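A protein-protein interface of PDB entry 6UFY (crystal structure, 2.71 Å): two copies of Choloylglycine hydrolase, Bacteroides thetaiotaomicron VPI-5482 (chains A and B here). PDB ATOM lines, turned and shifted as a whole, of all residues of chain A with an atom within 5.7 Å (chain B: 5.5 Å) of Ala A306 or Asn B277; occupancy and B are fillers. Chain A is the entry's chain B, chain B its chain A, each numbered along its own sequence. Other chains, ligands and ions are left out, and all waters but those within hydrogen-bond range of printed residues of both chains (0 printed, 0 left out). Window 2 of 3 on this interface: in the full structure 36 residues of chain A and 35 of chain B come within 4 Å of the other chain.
The backbone carbonyl oxygen (O) of Pro B276 is in hydrogen-bond range of the backbone NH (N) of Leu A278, 3.1 Å away. O of Pro A276 lies within hydrogen-bond range of N of Leu B278 (3.0 Å).
The side-chain amide nitrogen (ND2) of Asn A277 lies close to the backbone carbonyl oxygen (O) of Tyr A305 (3.3 Å).
Among the printed residues, pairs that only touch across the chains: Asn A277 with Asn B277 (3.2 Å), Ala A306 with Asn B277 (3.6 Å), Asn A277 with Leu B278 (3.8 Å), Pro A276 with Asn B277 (3.9 Å) and Asn A277 with Pro B276 (3.96 Å).
Ala A306 touches just one residue of chain B: Asn B277. Of chain A, only Pro A276, Asn A277 and Ala A306 come within 4 Å of Asn B277. Of the printed residues of chain A, Leu B278 touches Pro A276 and Asn A277. Printed residues of chain A within 4 Å of Pro B276: Asn A277 (3.96 Å) and Leu A278 (3.1 Å). Of the printed residues of chain B, Leu A278 touches Pro B276 (3.1 Å). Of the printed residues of chain B, Pro A276 touches Asn B277 and Leu B278. Phe A279 touches none of the printed residues of chain B. Tyr B305 touches none of the printed residues of chain A. The nearest residue of chain B that does not touch Ala A306 is Ala B306 (4.7 Å). The nearest residue of chain A that does not touch Asn B277 is Leu A278 (4.3 Å). The nearest printed residue of chain B that does not touch Leu A278 is Asn B277 (4.3 Å).
Of the 11 printed residues of chain B, 3 touch a printed residue of chain A. Hydrophobic or aromatic side chains of chain B that line the printed part of chain A: Pro B276 and Leu B278. Of the 11 printed residues of chain A, 4 touch a printed residue of chain B. Hydrophobic or aromatic side chains of chain A that line the printed part of chain B: Pro A276, Leu A278 and Ala A306. Among the printed residues, 7 pairs touch across the chains. Among the printed residues, no Asp or Glu carboxylate lies within 4 Å of a Lys or Arg side-chain nitrogen of the other chain.
Pro A276 touches Asn B277, and with the chains exchanged Asn A277 touches Pro B276. Pro A276 touches Leu B278, and with the chains exchanged Leu A278 touches Pro B276. Asn B277 touches its own counterpart, Asn A277. Ala A306 touches Asn B277, but with the chains exchanged Asn A277 does not touch Ala B306 (4.6 Å). 7 positions are printed for both chains. Of the 7 pairs that touch across the chains among the printed residues, 5 have their exchanged pair printed and touching as well.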
ATOM      1  N   PRO A 276       9.125  22.603   4.534  1.00  0.00           N
ATOM      2  CA  PRO A 276       9.362  22.119   5.902  1.00  0.00           C
ATOM      3  C   PRO A 276       8.398  21.047   6.380  1.00  0.00           C
ATOM      4  O   PRO A 276       8.696  20.385   7.383  1.00  0.00           O
ATOM      5  CB  PRO A 276       9.216  23.392   6.747  1.00  0.00           C
ATOM      6  CG  PRO A 276       8.229  24.213   5.983  1.00  0.00           C
ATOM      7  CD  PRO A 276       8.490  23.934   4.520  1.00  0.00           C
ATOM      8  N   ASN A 277       7.269  20.840   5.711  1.00  0.00           N
ATOM      9  CA  ASN A 277       6.202  20.018   6.261  1.00  0.00           C
ATOM     10  C   ASN A 277       6.028  18.721   5.481  1.00  0.00           C
ATOM     11  O   ASN A 277       6.406  18.610   4.310  1.00  0.00           O
ATOM     12  CB  ASN A 277       4.880  20.790   6.279  1.00  0.00           C
ATOM     13  CG  ASN A 277       4.997  22.130   6.979  1.00  0.00           C
ATOM     14  OD1 ASN A 277       5.907  22.349   7.777  1.00  0.00           O
ATOM     15  ND2 ASN A 277       4.070  23.034   6.683  1.00  0.00           N
ATOM     16  N   LEU A 278       5.442  17.735   6.158  1.00  0.00           N
ATOM     17  CA  LEU A 278       5.057  16.460   5.563  1.00  0.00           C
ATOM     18  C   LEU A 278       3.537  16.403   5.514  1.00  0.00           C
ATOM     19  O   LEU A 278       2.882  16.241   6.550  1.00  0.00           O
ATOM     20  CB  LEU A 278       5.622  15.284   6.358  1.00  0.00           C
ATOM     21  CG  LEU A 278       5.021  13.906   6.053  1.00  0.00           C
ATOM     22  CD1 LEU A 278       5.467  13.399   4.691  1.00  0.00           C
ATOM     23  CD2 LEU A 278       5.360  12.902   7.147  1.00  0.00           C
ATOM     24  N   PHE A 279       2.978  16.547   4.320  1.00  0.00           N
ATOM     25  CA  PHE A 279       1.543  16.446   4.117  1.00  0.00           C
ATOM     26  C   PHE A 279       1.189  15.073   3.558  1.00  0.00           C
ATOM     27  O   PHE A 279       2.056  14.279   3.187  1.00  0.00           O
ATOM     28  CB  PHE A 279       1.044  17.557   3.184  1.00  0.00           C
ATOM     29  CG  PHE A 279       1.721  17.575   1.842  1.00  0.00           C
ATOM     30  CD1 PHE A 279       1.224  16.826   0.789  1.00  0.00           C
ATOM     31  CD2 PHE A 279       2.848  18.350   1.632  1.00  0.00           C
ATOM     32  CE1 PHE A 279       1.842  16.843  -0.445  1.00  0.00           C
ATOM     33  CE2 PHE A 279       3.471  18.372   0.399  1.00  0.00           C
ATOM     34  CZ  PHE A 279       2.965  17.619  -0.639  1.00  0.00           C
ATOM     35  N   ILE A 304       3.193  25.574   0.423  1.00  0.00           N
ATOM     36  CA  ILE A 304       3.503  24.822   1.631  1.00  0.00           C
ATOM     37  C   ILE A 304       2.195  24.268   2.180  1.00  0.00           C
ATOM     38  O   ILE A 304       1.319  25.033   2.603  1.00  0.00           O
ATOM     39  CB  ILE A 304       4.213  25.691   2.677  1.00  0.00           C
ATOM     40  CG1 ILE A 304       5.471  26.319   2.075  1.00  0.00           C
ATOM     41  CG2 ILE A 304       4.557  24.866   3.909  1.00  0.00           C
ATOM     42  CD1 ILE A 304       5.739  27.730   2.553  1.00  0.00           C
ATOM     43  N   TYR A 305       2.060  22.947   2.174  1.00  0.00           N
ATOM     44  CA  TYR A 305       0.899  22.273   2.732  1.00  0.00           C
ATOM     45  C   TYR A 305       1.270  21.588   4.041  1.00  0.00           C
ATOM     46  O   TYR A 305       2.446  21.367   4.342  1.00  0.00           O
ATOM     47  CB  TYR A 305       0.329  21.243   1.752  1.00  0.00           C
ATOM     48  CG  TYR A 305      -0.009  21.811   0.396  1.00  0.00           C
ATOM     49  CD1 TYR A 305      -1.066  22.697   0.238  1.00  0.00           C
ATOM     50  CD2 TYR A 305       0.724  21.456  -0.727  1.00  0.00           C
ATOM     51  CE1 TYR A 305      -1.381  23.217  -1.002  1.00  0.00           C
ATOM     52  CE2 TYR A 305       0.417  21.969  -1.969  1.00  0.00           C
ATOM     53  CZ  TYR A 305      -0.636  22.850  -2.102  1.00  0.00           C
ATOM     54  OH  TYR A 305      -0.946  23.363  -3.340  1.00  0.00           O
ATOM     55  N   ALA A 306       0.245  21.248   4.821  1.00  0.00           N
ATOM     56  CA  ALA A 306       0.449  20.594   6.104  1.00  0.00           C
ATOM     57  C   ALA A 306      -0.738  19.689   6.400  1.00  0.00           C
ATOM     58  O   ALA A 306      -1.877  20.018   6.059  1.00  0.00           O
ATOM     59  CB  ALA A 306       0.635  21.616   7.231  1.00  0.00           C
ATOM     60  N   GLY A 307      -0.462  18.550   7.034  1.00  0.00           N
ATOM     61  CA  GLY A 307      -1.527  17.612   7.356  1.00  0.00           C
ATOM     62  C   GLY A 307      -2.169  17.040   6.106  1.00  0.00           C
ATOM     63  O   GLY A 307      -1.498  16.739   5.113  1.00  0.00           O
ATOM     64  N   ASP A 308      -3.490  16.884   6.155  1.00  0.00           N
ATOM     65  CA  ASP A 308      -4.243  16.404   5.002  1.00  0.00           C
ATOM     66  C   ASP A 308      -4.430  17.532   3.995  1.00  0.00           C
ATOM     67  O   ASP A 308      -4.931  18.608   4.340  1.00  0.00           O
ATOM     68  CB  ASP A 308      -5.602  15.857   5.440  1.00  0.00           C
ATOM     69  CG  ASP A 308      -6.432  15.347   4.275  1.00  0.00           C
ATOM     70  OD1 ASP A 308      -5.847  14.977   3.233  1.00  0.00           O
ATOM     71  OD2 ASP A 308      -7.674  15.322   4.402  1.00  0.00           O
ATOM     72  N   ALA A 309      -4.033  17.282   2.750  1.00  0.00           N
ATOM     73  CA  ALA A 309      -4.111  18.277   1.691  1.00  0.00           C
ATOM     74  C   ALA A 309      -5.316  18.079   0.778  1.00  0.00           C
ATOM     75  O   ALA A 309      -5.391  18.724  -0.273  1.00  0.00           O
ATOM     76  CB  ALA A 309      -2.824  18.271   0.867  1.00  0.00           C
ATOM     77  N   ASP A 312      -6.890  21.207   0.153  1.00  0.00           N
ATOM     78  CA  ASP A 312      -6.197  22.049  -0.808  1.00  0.00           C
ATOM     79  C   ASP A 312      -6.260  21.502  -2.229  1.00  0.00           C
ATOM     80  O   ASP A 312      -5.575  22.025  -3.113  1.00  0.00           O
ATOM     81  CB  ASP A 312      -4.743  22.228  -0.376  1.00  0.00           C
ATOM     82  CG  ASP A 312      -4.621  22.680   1.065  1.00  0.00           C
ATOM     83  OD1 ASP A 312      -5.206  23.729   1.410  1.00  0.00           O
ATOM     84  OD2 ASP A 312      -3.962  21.976   1.860  1.00  0.00           O
ATOM     85  N   PHE B 270      13.121  23.438  14.544  1.00  0.00           N
ATOM     86  CA  PHE B 270      13.005  22.244  15.368  1.00  0.00           C
ATOM     87  C   PHE B 270      12.063  21.263  14.688  1.00  0.00           C
ATOM     88  O   PHE B 270      11.049  21.667  14.114  1.00  0.00           O
ATOM     89  CB  PHE B 270      12.496  22.590  16.774  1.00  0.00           C
ATOM     90  CG  PHE B 270      12.696  21.495  17.784  1.00  0.00           C
ATOM     91  CD1 PHE B 270      11.775  20.469  17.909  1.00  0.00           C
ATOM     92  CD2 PHE B 270      13.801  21.500  18.619  1.00  0.00           C
ATOM     93  CE1 PHE B 270      11.955  19.465  18.840  1.00  0.00           C
ATOM     94  CE2 PHE B 270      13.986  20.499  19.553  1.00  0.00           C
ATOM     95  CZ  PHE B 270      13.061  19.481  19.663  1.00  0.00           C
ATOM     96  N   GLU B 271      12.403  19.977  14.761  1.00  0.00           N
ATOM     97  CA  GLU B 271      11.594  18.925  14.159  1.00  0.00           C
ATOM     98  C   GLU B 271      11.730  17.656  14.985  1.00  0.00           C
ATOM     99  O   GLU B 271      12.840  17.275  15.365  1.00  0.00           O
ATOM    100  CB  GLU B 271      12.018  18.644  12.713  1.00  0.00           C
ATOM    101  CG  GLU B 271      11.381  17.398  12.119  1.00  0.00           C
ATOM    102  CD  GLU B 271      12.268  16.717  11.099  1.00  0.00           C
ATOM    103  OE1 GLU B 271      12.873  17.423  10.265  1.00  0.00           O
ATOM    104  OE2 GLU B 271      12.369  15.471  11.139  1.00  0.00           O
ATOM    105  N   SER B 272      10.603  17.007  15.252  1.00  0.00           N
ATOM    106  CA  SER B 272      10.589  15.704  15.898  1.00  0.00           C
ATOM    107  C   SER B 272      10.374  14.614  14.856  1.00  0.00           C
ATOM    108  O   SER B 272       9.688  14.817  13.851  1.00  0.00           O
ATOM    109  CB  SER B 272       9.501  15.630  16.971  1.00  0.00           C
ATOM    110  OG  SER B 272       9.688  16.630  17.958  1.00  0.00           O
ATOM    111  N   THR B 275       6.753  13.496  14.485  1.00  0.00           N
ATOM    112  CA  THR B 275       5.825  14.530  14.053  1.00  0.00           C
ATOM    113  C   THR B 275       6.157  14.964  12.628  1.00  0.00           C
ATOM    114  O   THR B 275       7.335  15.017  12.258  1.00  0.00           O
ATOM    115  CB  THR B 275       5.857  15.756  14.979  1.00  0.00           C
ATOM    116  OG1 THR B 275       7.172  16.322  14.992  1.00  0.00           O
ATOM    117  CG2 THR B 275       5.454  15.367  16.395  1.00  0.00           C
ATOM    118  N   PRO B 276       5.149  15.277  11.808  1.00  0.00           N
ATOM    119  CA  PRO B 276       5.411  15.473  10.374  1.00  0.00           C
ATOM    120  C   PRO B 276       6.013  16.820  10.005  1.00  0.00           C
ATOM    121  O   PRO B 276       6.646  16.913   8.945  1.00  0.00           O
ATOM    122  CB  PRO B 276       4.022  15.309   9.743  1.00  0.00           C
ATOM    123  CG  PRO B 276       3.081  15.743  10.815  1.00  0.00           C
ATOM    124  CD  PRO B 276       3.710  15.331  12.123  1.00  0.00           C
ATOM    125  N   ASN B 277       5.853  17.857  10.820  1.00  0.00           N
ATOM    126  CA  ASN B 277       6.195  19.211  10.405  1.00  0.00           C
ATOM    127  C   ASN B 277       7.500  19.685  11.037  1.00  0.00           C
ATOM    128  O   ASN B 277       7.888  19.244  12.123  1.00  0.00           O
ATOM    129  CB  ASN B 277       5.071  20.188  10.760  1.00  0.00           C
ATOM    130  CG  ASN B 277       3.736  19.784  10.163  1.00  0.00           C
ATOM    131  OD1 ASN B 277       3.420  20.136   9.027  1.00  0.00           O
ATOM    132  ND2 ASN B 277       2.945  19.046  10.931  1.00  0.00           N
ATOM    133  N   LEU B 278       8.172  20.598  10.336  1.00  0.00           N
ATOM    134  CA  LEU B 278       9.348  21.301  10.840  1.00  0.00           C
ATOM    135  C   LEU B 278       8.927  22.724  11.182  1.00  0.00           C
ATOM    136  O   LEU B 278       8.706  23.545  10.284  1.00  0.00           O
ATOM    137  CB  LEU B 278      10.478  21.294   9.812  1.00  0.00           C
ATOM    138  CG  LEU B 278      11.629  22.282  10.028  1.00  0.00           C
ATOM    139  CD1 LEU B 278      12.634  21.754  11.039  1.00  0.00           C
ATOM    140  CD2 LEU B 278      12.310  22.617   8.709  1.00  0.00           C
ATOM    141  N   PHE B 279       8.804  23.013  12.472  1.00  0.00           N
ATOM    142  CA  PHE B 279       8.438  24.341  12.939  1.00  0.00           C
ATOM    143  C   PHE B 279       9.680  25.105  13.383  1.00  0.00           C
ATOM    144  O   PHE B 279      10.791  24.570  13.426  1.00  0.00           O
ATOM    145  CB  PHE B 279       7.419  24.252  14.080  1.00  0.00           C
ATOM    146  CG  PHE B 279       7.905  23.479  15.271  1.00  0.00           C
ATOM    147  CD1 PHE B 279       7.723  22.107  15.345  1.00  0.00           C
ATOM    148  CD2 PHE B 279       8.536  24.123  16.324  1.00  0.00           C
ATOM    149  CE1 PHE B 279       8.168  21.393  16.440  1.00  0.00           C
ATOM    150  CE2 PHE B 279       8.983  23.415  17.421  1.00  0.00           C
ATOM    151  CZ  PHE B 279       8.797  22.048  17.479  1.00  0.00           C
ATOM    152  N   ILE B 304       1.373  18.842  17.697  1.00  0.00           N
ATOM    153  CA  ILE B 304       1.824  19.051  16.325  1.00  0.00           C
ATOM    154  C   ILE B 304       1.777  20.542  16.029  1.00  0.00           C
ATOM    155  O   ILE B 304       0.700  21.152  16.040  1.00  0.00           O
ATOM    156  CB  ILE B 304       0.969  18.262  15.322  1.00  0.00           C
ATOM    157  CG1 ILE B 304       1.026  16.766  15.637  1.00  0.00           C
ATOM    158  CG2 ILE B 304       1.426  18.536  13.896  1.00  0.00           C
ATOM    159  CD1 ILE B 304       0.132  15.922  14.761  1.00  0.00           C
ATOM    160  N   TYR B 305       2.940  21.129  15.766  1.00  0.00           N
ATOM    161  CA  TYR B 305       3.060  22.528  15.390  1.00  0.00           C
ATOM    162  C   TYR B 305       3.570  22.636  13.959  1.00  0.00           C
ATOM    163  O   TYR B 305       4.145  21.694  13.409  1.00  0.00           O
ATOM    164  CB  TYR B 305       4.000  23.276  16.343  1.00  0.00           C
ATOM    165  CG  TYR B 305       3.678  23.063  17.804  1.00  0.00           C
ATOM    166  CD1 TYR B 305       2.600  23.706  18.399  1.00  0.00           C
ATOM    167  CD2 TYR B 305       4.452  22.220  18.588  1.00  0.00           C
ATOM    168  CE1 TYR B 305       2.302  23.513  19.734  1.00  0.00           C
ATOM    169  CE2 TYR B 305       4.162  22.022  19.923  1.00  0.00           C
ATOM    170  CZ  TYR B 305       3.087  22.670  20.492  1.00  0.00           C
ATOM    171  OH  TYR B 305       2.798  22.473  21.823  1.00  0.00           O
ATOM    172  N   ALA B 306       3.357  23.805  13.357  1.00  0.00           N
ATOM    173  CA  ALA B 306       3.744  24.019  11.971  1.00  0.00           C
ATOM    174  C   ALA B 306       4.065  25.489  11.751  1.00  0.00           C
ATOM    175  O   ALA B 306       3.450  26.371  12.355  1.00  0.00           O
ATOM    176  CB  ALA B 306       2.644  23.568  11.003  1.00  0.00           C
